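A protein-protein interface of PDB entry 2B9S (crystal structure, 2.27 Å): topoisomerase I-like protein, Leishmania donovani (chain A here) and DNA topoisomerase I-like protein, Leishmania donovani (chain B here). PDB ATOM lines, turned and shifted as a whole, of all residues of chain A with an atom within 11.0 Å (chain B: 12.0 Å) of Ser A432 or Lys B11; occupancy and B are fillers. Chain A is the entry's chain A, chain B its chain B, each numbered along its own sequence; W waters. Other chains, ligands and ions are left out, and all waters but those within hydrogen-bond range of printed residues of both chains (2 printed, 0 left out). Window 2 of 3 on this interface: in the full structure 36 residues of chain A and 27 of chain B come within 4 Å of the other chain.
Among the printed residues, pairs that only touch across the chains: Ile A331 with Lys B11 (3.9 Å), Thr A421 with Leu B15 (3.6 Å), Ala A424 with Val B13 (3.5 Å), Ala A424 with Ser B14 (3.2 Å), His A429 with Val B13 (3.5 Å), His A429 with Thr B17 (3.5 Å), Gln A430 with Lys B11 (3.2 Å), Gln A430 with Ala B12 (3.1 Å), Gln A430 with Ser B14 (3.6 Å), Lys A431 with Lys B11 (3.4 Å), Lys A431 with Ser B14 (3.9 Å) and Ser A432 with Lys B11 (3.7 Å).
The backbone carbonyl oxygen of Arg A332 lies within hydrogen-bond range of the side-chain amide nitrogen of Gln A430. OD1 of Asn A428 lies within hydrogen-bond range of NE2 of Gln A430, at 3.0 Å. N of His A429 lies within hydrogen-bond range of O of Ala A424 (3.0 Å).
Water W2 lies within hydrogen-bond range of OG of Ser B14 (2.6 Å) and O of Gln A430 (3.0 Å). Water W1 lies within hydrogen-bond range of O of Ser B14, ND1 of His A429 and O of Leu B15.
Ser A432 touches one residue of chain B. Printed residues of chain A within 4 Å of Lys B11: Ile A331 (3.9 Å), Gln A430 (3.2 Å), Lys A431 (3.4 Å) and Ser A432 (3.7 Å). Of chain B, only Lys B11 (3.2 Å), Ala B12 (3.1 Å) and Ser B14 (3.6 Å) come within 4 Å of Gln A430. Of the printed residues of chain B, Lys A431 touches Lys B11, Ala B12 and Ser B14. Ala B12 touches just these residues of chain A: Gln A430 (3.1 Å) and Lys A431 (2.8 Å). Of the printed residues of chain B, Ala A424 touches Val B13 (3.5 Å) and Ser B14 (3.2 Å). Printed residues of chain B within 4 Å of Thr A421: Leu B15. Of the printed residues of chain A, Val B13 touches Ala A424 (3.5 Å) and His A429 (3.5 Å). Printed residues of chain A within 4 Å of Leu B15: Thr A421. Gln A334 touches none of the printed residues of chain B.
The backbone carbonyl oxygen (O) of Ala B12 sits at hydrogen-bond distance from the backbone NH (N) of Lys A431 (2.8 Å). The backbone NH of Ser B14 is in hydrogen-bond range of the backbone carbonyl oxygen of His A429, 2.9 Å away.
Of the 23 printed residues of chain A, 7 touch a printed residue of chain B. Of the 7 printed residues of chain B, 6 touch a printed residue of chain A. Hydrophobic or aromatic side chains of chain B that line the printed part of chain A: Val B13 and Leu B15. Among the printed residues, no Asp or Glu carboxylate lies within 4 Å of a Lys or Arg side-chain nitrogen of the other chain.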
ATOM      1  N   HIS A  69       7.821  22.820  34.796  1.00  0.00           N
ATOM      2  CA  HIS A  69       6.489  22.734  34.215  1.00  0.00           C
ATOM      3  C   HIS A  69       5.455  23.306  35.171  1.00  0.00           C
ATOM      4  O   HIS A  69       5.600  23.156  36.382  1.00  0.00           O
ATOM      5  CB  HIS A  69       6.121  21.285  33.889  1.00  0.00           C
ATOM      6  CG  HIS A  69       5.102  21.179  32.801  1.00  0.00           C
ATOM      7  ND1 HIS A  69       3.763  21.415  33.015  1.00  0.00           N
ATOM      8  CD2 HIS A  69       5.236  20.927  31.477  1.00  0.00           C
ATOM      9  CE1 HIS A  69       3.114  21.315  31.868  1.00  0.00           C
ATOM     10  NE2 HIS A  69       3.985  21.007  30.920  1.00  0.00           N
ATOM     11  N   ASP A  70       4.413  23.939  34.626  1.00  0.00           N
ATOM     12  CA  ASP A  70       3.278  24.474  35.421  1.00  0.00           C
ATOM     13  C   ASP A  70       2.603  23.441  36.320  1.00  0.00           C
ATOM     14  O   ASP A  70       2.158  23.772  37.408  1.00  0.00           O
ATOM     15  CB  ASP A  70       2.196  25.085  34.509  1.00  0.00           C
ATOM     16  CG  ASP A  70       2.642  26.400  33.833  1.00  0.00           C
ATOM     17  OD1 ASP A  70       3.720  26.943  34.164  1.00  0.00           O
ATOM     18  OD2 ASP A  70       1.897  26.890  32.952  1.00  0.00           O
ATOM     19  N   ARG A 166      -6.002  17.581  31.293  1.00  0.00           N
ATOM     20  CA  ARG A 166      -6.300  18.906  30.776  1.00  0.00           C
ATOM     21  C   ARG A 166      -7.193  19.681  31.733  1.00  0.00           C
ATOM     22  O   ARG A 166      -8.073  19.114  32.377  1.00  0.00           O
ATOM     23  CB  ARG A 166      -7.018  18.786  29.421  1.00  0.00           C
ATOM     24  CG  ARG A 166      -6.280  18.010  28.331  1.00  0.00           C
ATOM     25  CD  ARG A 166      -4.974  18.627  27.919  1.00  0.00           C
ATOM     26  NE  ARG A 166      -4.375  17.862  26.811  1.00  0.00           N
ATOM     27  CZ  ARG A 166      -4.526  18.129  25.509  1.00  0.00           C
ATOM     28  NH1 ARG A 166      -5.242  19.164  25.098  1.00  0.00           N
ATOM     29  NH2 ARG A 166      -3.960  17.335  24.611  1.00  0.00           N
ATOM     30  N   GLY A 167      -7.005  20.987  31.781  1.00  0.00           N
ATOM     31  CA  GLY A 167      -7.776  21.865  32.655  1.00  0.00           C
ATOM     32  C   GLY A 167      -7.717  21.485  34.128  1.00  0.00           C
ATOM     33  O   GLY A 167      -6.660  21.131  34.653  1.00  0.00           O
ATOM     34  N   LYS A 168      -8.849  21.577  34.803  1.00  0.00           N
ATOM     35  CA  LYS A 168      -8.917  21.271  36.212  1.00  0.00           C
ATOM     36  C   LYS A 168      -9.310  19.817  36.427  1.00  0.00           C
ATOM     37  O   LYS A 168     -10.358  19.510  36.993  1.00  0.00           O
ATOM     38  CB  LYS A 168      -9.873  22.254  36.934  1.00  0.00           C
ATOM     39  N   PHE A 325     -18.465  29.132  28.603  1.00  0.00           N
ATOM     40  CA  PHE A 325     -18.296  27.810  29.226  1.00  0.00           C
ATOM     41  C   PHE A 325     -17.053  27.097  28.733  1.00  0.00           C
ATOM     42  O   PHE A 325     -16.547  27.387  27.642  1.00  0.00           O
ATOM     43  CB  PHE A 325     -19.558  26.942  29.016  1.00  0.00           C
ATOM     44  CG  PHE A 325     -19.802  26.537  27.584  1.00  0.00           C
ATOM     45  CD1 PHE A 325     -19.127  25.444  27.027  1.00  0.00           C
ATOM     46  CD2 PHE A 325     -20.723  27.234  26.792  1.00  0.00           C
ATOM     47  CE1 PHE A 325     -19.353  25.052  25.675  1.00  0.00           C
ATOM     48  CE2 PHE A 325     -20.956  26.873  25.446  1.00  0.00           C
ATOM     49  CZ  PHE A 325     -20.272  25.770  24.889  1.00  0.00           C
ATOM     50  N   LEU A 326     -16.565  26.149  29.529  1.00  0.00           N
ATOM     51  CA  LEU A 326     -15.464  25.284  29.098  1.00  0.00           C
ATOM     52  C   LEU A 326     -16.057  24.053  28.435  1.00  0.00           C
ATOM     53  O   LEU A 326     -16.909  23.358  29.016  1.00  0.00           O
ATOM     54  CB  LEU A 326     -14.550  24.903  30.284  1.00  0.00           C
ATOM     55  CG  LEU A 326     -13.921  26.062  31.091  1.00  0.00           C
ATOM     56  CD1 LEU A 326     -13.110  25.511  32.250  1.00  0.00           C
ATOM     57  CD2 LEU A 326     -13.046  27.003  30.233  1.00  0.00           C
ATOM     58  N   GLY A 327     -15.621  23.787  27.211  1.00  0.00           N
ATOM     59  CA  GLY A 327     -16.067  22.606  26.486  1.00  0.00           C
ATOM     60  C   GLY A 327     -14.994  21.542  26.472  1.00  0.00           C
ATOM     61  O   GLY A 327     -14.076  21.564  27.298  1.00  0.00           O
ATOM     62  N   LYS A 328     -15.098  20.611  25.527  1.00  0.00           N
ATOM     63  CA  LYS A 328     -14.078  19.577  25.352  1.00  0.00           C
ATOM     64  C   LYS A 328     -12.654  20.150  25.407  1.00  0.00           C
ATOM     65  O   LYS A 328     -12.357  21.162  24.753  1.00  0.00           O
ATOM     66  CB  LYS A 328     -14.294  18.827  24.030  1.00  0.00           C
ATOM     67  CG  LYS A 328     -13.179  17.836  23.706  1.00  0.00           C
ATOM     68  CD  LYS A 328     -13.536  16.984  22.517  1.00  0.00           C
ATOM     69  CE  LYS A 328     -12.427  16.017  22.178  1.00  0.00           C
ATOM     70  NZ  LYS A 328     -12.687  15.461  20.800  1.00  0.00           N
ATOM     71  N   ASP A 329     -11.788  19.484  26.174  1.00  0.00           N
ATOM     72  CA  ASP A 329     -10.379  19.893  26.366  1.00  0.00           C
ATOM     73  C   ASP A 329     -10.203  21.152  27.222  1.00  0.00           C
ATOM     74  O   ASP A 329      -9.084  21.666  27.363  1.00  0.00           O
ATOM     75  CB  ASP A 329      -9.633  20.006  25.028  1.00  0.00           C
ATOM     76  CG  ASP A 329      -9.220  18.649  24.484  1.00  0.00           C
ATOM     77  OD1 ASP A 329      -9.724  18.258  23.424  1.00  0.00           O
ATOM     78  OD2 ASP A 329      -8.424  17.949  25.132  1.00  0.00           O
ATOM     79  N   SER A 330     -11.312  21.603  27.828  1.00  0.00           N
ATOM     80  CA  SER A 330     -11.349  22.773  28.705  1.00  0.00           C
ATOM     81  C   SER A 330     -11.029  24.034  27.922  1.00  0.00           C
ATOM     82  O   SER A 330     -10.533  25.029  28.474  1.00  0.00           O
ATOM     83  CB  SER A 330     -10.435  22.597  29.939  1.00  0.00           C
ATOM     84  OG  SER A 330     -10.932  21.548  30.746  1.00  0.00           O
ATOM     85  N   ILE A 331     -11.345  23.980  26.631  1.00  0.00           N
ATOM     86  CA  ILE A 331     -11.260  25.143  25.747  1.00  0.00           C
ATOM     87  C   ILE A 331     -12.514  25.949  25.979  1.00  0.00           C
ATOM     88  O   ILE A 331     -13.622  25.409  25.972  1.00  0.00           O
ATOM     89  CB  ILE A 331     -11.122  24.728  24.234  1.00  0.00           C
ATOM     90  CG1 ILE A 331      -9.866  23.858  23.992  1.00  0.00           C
ATOM     91  CG2 ILE A 331     -11.183  25.941  23.297  1.00  0.00           C
ATOM     92  CD1 ILE A 331      -8.533  24.425  24.525  1.00  0.00           C
ATOM     93  N   ARG A 332     -12.325  27.239  26.222  1.00  0.00           N
ATOM     94  CA  ARG A 332     -13.407  28.144  26.536  1.00  0.00           C
ATOM     95  C   ARG A 332     -14.204  28.510  25.289  1.00  0.00           C
ATOM     96  O   ARG A 332     -13.647  28.771  24.234  1.00  0.00           O
ATOM     97  CB  ARG A 332     -12.843  29.399  27.222  1.00  0.00           C
ATOM     98  CG  ARG A 332     -13.882  30.358  27.777  1.00  0.00           C
ATOM     99  CD  ARG A 332     -13.186  31.542  28.389  1.00  0.00           C
ATOM    100  NE  ARG A 332     -14.105  32.464  29.068  1.00  0.00           N
ATOM    101  CZ  ARG A 332     -13.720  33.487  29.835  1.00  0.00           C
ATOM    102  NH1 ARG A 332     -12.431  33.725  30.034  1.00  0.00           N
ATOM    103  NH2 ARG A 332     -14.622  34.280  30.406  1.00  0.00           N
ATOM    104  N   TYR A 333     -15.522  28.466  25.416  1.00  0.00           N
ATOM    105  CA  TYR A 333     -16.407  28.905  24.367  1.00  0.00           C
ATOM    106  C   TYR A 333     -17.041  30.213  24.848  1.00  0.00           C
ATOM    107  O   TYR A 333     -17.720  30.230  25.881  1.00  0.00           O
ATOM    108  CB  TYR A 333     -17.463  27.832  24.083  1.00  0.00           C
ATOM    109  CG  TYR A 333     -18.410  28.186  22.959  1.00  0.00           C
ATOM    110  CD1 TYR A 333     -19.508  29.024  23.191  1.00  0.00           C
ATOM    111  CD2 TYR A 333     -18.216  27.694  21.671  1.00  0.00           C
ATOM    112  CE1 TYR A 333     -20.383  29.357  22.194  1.00  0.00           C
ATOM    113  CE2 TYR A 333     -19.094  28.027  20.648  1.00  0.00           C
ATOM    114  CZ  TYR A 333     -20.187  28.865  20.923  1.00  0.00           C
ATOM    115  OH  TYR A 333     -21.087  29.229  19.944  1.00  0.00           O
ATOM    116  N   GLN A 334     -16.788  31.292  24.105  1.00  0.00           N
ATOM    117  CA  GLN A 334     -17.337  32.615  24.374  1.00  0.00           C
ATOM    118  C   GLN A 334     -17.978  33.105  23.099  1.00  0.00           C
ATOM    119  O   GLN A 334     -17.316  33.198  22.063  1.00  0.00           O
ATOM    120  CB  GLN A 334     -16.239  33.597  24.782  1.00  0.00           C
ATOM    121  CG  GLN A 334     -15.826  33.503  26.235  1.00  0.00           C
ATOM    122  CD  GLN A 334     -14.687  34.445  26.583  1.00  0.00           C
ATOM    123  OE1 GLN A 334     -13.550  34.271  26.132  1.00  0.00           O
ATOM    124  NE2 GLN A 334     -14.979  35.428  27.411  1.00  0.00           N
ATOM    125  N   THR A 421     -10.019  29.672   8.550  1.00  0.00           N
ATOM    126  CA  THR A 421     -10.153  30.414   9.819  1.00  0.00           C
ATOM    127  C   THR A 421     -11.627  30.566  10.199  1.00  0.00           C
ATOM    128  O   THR A 421     -11.978  30.433  11.365  1.00  0.00           O
ATOM    129  CB  THR A 421      -9.465  31.821   9.748  1.00  0.00           C
ATOM    130  OG1 THR A 421      -8.060  31.668   9.529  1.00  0.00           O
ATOM    131  CG2 THR A 421      -9.666  32.659  11.038  1.00  0.00           C
ATOM    132  N   ALA A 424     -12.651  27.195  11.578  1.00  0.00           N
ATOM    133  CA  ALA A 424     -12.039  26.981  12.883  1.00  0.00           C
ATOM    134  C   ALA A 424     -12.700  27.789  14.010  1.00  0.00           C
ATOM    135  O   ALA A 424     -12.804  27.304  15.147  1.00  0.00           O
ATOM    136  CB  ALA A 424     -10.547  27.274  12.810  1.00  0.00           C
ATOM    137  N   ILE A 425     -13.141  29.011  13.701  1.00  0.00           N
ATOM    138  CA  ILE A 425     -13.880  29.861  14.660  1.00  0.00           C
ATOM    139  C   ILE A 425     -15.243  29.264  15.031  1.00  0.00           C
ATOM    140  O   ILE A 425     -15.591  29.205  16.216  1.00  0.00           O
ATOM    141  CB  ILE A 425     -14.024  31.324  14.154  1.00  0.00           C
ATOM    142  CG1 ILE A 425     -12.737  32.096  14.439  1.00  0.00           C
ATOM    143  CG2 ILE A 425     -15.240  32.039  14.794  1.00  0.00           C
ATOM    144  CD1 ILE A 425     -12.565  33.354  13.613  1.00  0.00           C
ATOM    145  N   ASN A 428     -14.545  26.375  17.179  1.00  0.00           N
ATOM    146  CA  ASN A 428     -13.860  26.830  18.394  1.00  0.00           C
ATOM    147  C   ASN A 428     -12.547  26.077  18.667  1.00  0.00           C
ATOM    148  O   ASN A 428     -12.175  25.775  19.821  1.00  0.00           O
ATOM    149  CB  ASN A 428     -14.815  26.833  19.595  1.00  0.00           C
ATOM    150  CG  ASN A 428     -14.321  27.693  20.725  1.00  0.00           C
ATOM    151  OD1 ASN A 428     -13.767  28.780  20.513  1.00  0.00           O
ATOM    152  ND2 ASN A 428     -14.493  27.199  21.953  1.00  0.00           N
ATOM    153  N   HIS A 429     -11.834  25.808  17.583  1.00  0.00           N
ATOM    154  CA  HIS A 429     -10.520  25.182  17.643  1.00  0.00           C
ATOM    155  C   HIS A 429      -9.425  26.187  18.000  1.00  0.00           C
ATOM    156  O   HIS A 429      -9.303  27.241  17.369  1.00  0.00           O
ATOM    157  CB  HIS A 429     -10.241  24.456  16.328  1.00  0.00           C
ATOM    158  CG  HIS A 429     -11.169  23.300  16.072  1.00  0.00           C
ATOM    159  ND1 HIS A 429     -11.485  22.864  14.805  1.00  0.00           N
ATOM    160  CD2 HIS A 429     -11.837  22.484  16.929  1.00  0.00           C
ATOM    161  CE1 HIS A 429     -12.292  21.818  14.892  1.00  0.00           C
ATOM    162  NE2 HIS A 429     -12.536  21.580  16.170  1.00  0.00           N
ATOM    163  N   GLN A 430      -8.666  25.865  19.050  1.00  0.00           N
ATOM    164  CA  GLN A 430      -7.703  26.776  19.655  1.00  0.00           C
ATOM    165  C   GLN A 430      -6.359  26.123  19.992  1.00  0.00           C
ATOM    166  O   GLN A 430      -6.280  24.934  20.295  1.00  0.00           O
ATOM    167  CB  GLN A 430      -8.283  27.399  20.919  1.00  0.00           C
ATOM    168  CG  GLN A 430      -9.464  28.297  20.688  1.00  0.00           C
ATOM    169  CD  GLN A 430      -9.941  28.919  21.963  1.00  0.00           C
ATOM    170  OE1 GLN A 430      -9.186  29.029  22.934  1.00  0.00           O
ATOM    171  NE2 GLN A 430     -11.209  29.305  21.993  1.00  0.00           N
ATOM    172  N   LYS A 431      -5.300  26.926  19.925  1.00  0.00           N
ATOM    173  CA  LYS A 431      -3.937  26.474  20.182  1.00  0.00           C
ATOM    174  C   LYS A 431      -3.331  27.476  21.154  1.00  0.00           C
ATOM    175  O   LYS A 431      -3.568  28.678  21.047  1.00  0.00           O
ATOM    176  CB  LYS A 431      -3.119  26.430  18.856  1.00  0.00           C
ATOM    177  N   SER A 432      -2.558  27.005  22.112  1.00  0.00           N
ATOM    178  CA  SER A 432      -1.891  27.946  22.985  1.00  0.00           C
ATOM    179  C   SER A 432      -0.429  28.087  22.543  1.00  0.00           C
ATOM    180  O   SER A 432      -0.057  29.021  21.807  1.00  0.00           O
ATOM    181  CB  SER A 432      -2.050  27.568  24.465  1.00  0.00           C
ATOM    182  OG  SER A 432      -1.073  26.630  24.880  1.00  0.00           O
ATOM    183  OXT SER A 432       0.412  27.261  22.891  1.00  0.00           O
ATOM    184  N   LYS B  11      -4.431  32.373  23.709  1.00  0.00           N
ATOM    185  CA  LYS B  11      -4.862  31.281  22.781  1.00  0.00           C
ATOM    186  C   LYS B  11      -5.231  31.778  21.392  1.00  0.00           C
ATOM    187  O   LYS B  11      -5.964  32.744  21.244  1.00  0.00           O
ATOM    188  CB  LYS B  11      -6.020  30.489  23.372  1.00  0.00           C
ATOM    189  CG  LYS B  11      -5.563  29.425  24.312  1.00  0.00           C
ATOM    190  CD  LYS B  11      -6.335  28.156  24.103  1.00  0.00           C
ATOM    191  CE  LYS B  11      -5.656  27.007  24.809  1.00  0.00           C
ATOM    192  NZ  LYS B  11      -5.387  27.340  26.252  1.00  0.00           N
ATOM    193  N   ALA B  12      -4.727  31.095  20.377  1.00  0.00           N
ATOM    194  CA  ALA B  12      -4.988  31.463  18.998  1.00  0.00           C
ATOM    195  C   ALA B  12      -5.925  30.452  18.337  1.00  0.00           C
ATOM    196  O   ALA B  12      -6.072  29.331  18.815  1.00  0.00           O
ATOM    197  CB  ALA B  12      -3.665  31.559  18.235  1.00  0.00           C
ATOM    198  N   VAL B  13      -6.556  30.872  17.247  1.00  0.00           N
ATOM    199  CA  VAL B  13      -7.368  30.011  16.387  1.00  0.00           C
ATOM    200  C   VAL B  13      -6.466  28.914  15.778  1.00  0.00           C
ATOM    201  O   VAL B  13      -5.317  29.171  15.369  1.00  0.00           O
ATOM    202  CB  VAL B  13      -8.085  30.850  15.261  1.00  0.00           C
ATOM    203  CG1 VAL B  13      -9.025  30.001  14.405  1.00  0.00           C
ATOM    204  CG2 VAL B  13      -8.860  32.006  15.869  1.00  0.00           C
ATOM    205  N   SER B  14      -6.997  27.694  15.734  1.00  0.00           N
ATOM    206  CA  SER B  14      -6.248  26.539  15.283  1.00  0.00           C
ATOM    207  C   SER B  14      -6.927  25.996  14.037  1.00  0.00           C
ATOM    208  O   SER B  14      -8.109  25.625  14.061  1.00  0.00           O
ATOM    209  CB  SER B  14      -6.195  25.494  16.397  1.00  0.00           C
ATOM    210  OG  SER B  14      -5.240  24.485  16.142  1.00  0.00           O
ATOM    211  N   LEU B  15      -6.177  25.956  12.943  1.00  0.00           N
ATOM    212  CA  LEU B  15      -6.752  25.631  11.647  1.00  0.00           C
ATOM    213  C   LEU B  15      -6.655  24.140  11.292  1.00  0.00           C
ATOM    214  O   LEU B  15      -7.404  23.647  10.423  1.00  0.00           O
ATOM    215  CB  LEU B  15      -6.112  26.508  10.551  1.00  0.00           C
ATOM    216  CG  LEU B  15      -6.692  27.882  10.173  1.00  0.00           C
ATOM    217  CD1 LEU B  15      -6.830  28.857  11.347  1.00  0.00           C
ATOM    218  CD2 LEU B  15      -5.800  28.480   9.079  1.00  0.00           C
ATOM    219  N   GLY B  16      -5.767  23.431  11.995  1.00  0.00           N
ATOM    220  CA  GLY B  16      -5.480  22.018  11.726  1.00  0.00           C
ATOM    221  C   GLY B  16      -6.635  21.060  11.952  1.00  0.00           C
ATOM    222  O   GLY B  16      -6.982  20.268  11.068  1.00  0.00           O
ATOM    223  N   THR B  17      -7.242  21.143  13.133  1.00  0.00           N
ATOM    224  CA  THR B  17      -8.305  20.223  13.540  1.00  0.00           C
ATOM    225  C   THR B  17      -9.439  20.103  12.518  1.00  0.00           C
ATOM    226  O   THR B  17      -9.880  18.998  12.220  1.00  0.00           O
ATOM    227  CB  THR B  17      -8.844  20.639  14.918  1.00  0.00           C
ATOM    228  OG1 THR B  17      -7.733  21.036  15.716  1.00  0.00           O
ATOM    229  CG2 THR B  17      -9.608  19.484  15.636  1.00  0.00           C
HETATM  230  O   HOH W   1      -9.745  23.877  12.881  1.00  0.00           O
HETATM  231  O   HOH W   2      -5.639  22.908  18.118  1.00  0.00           O
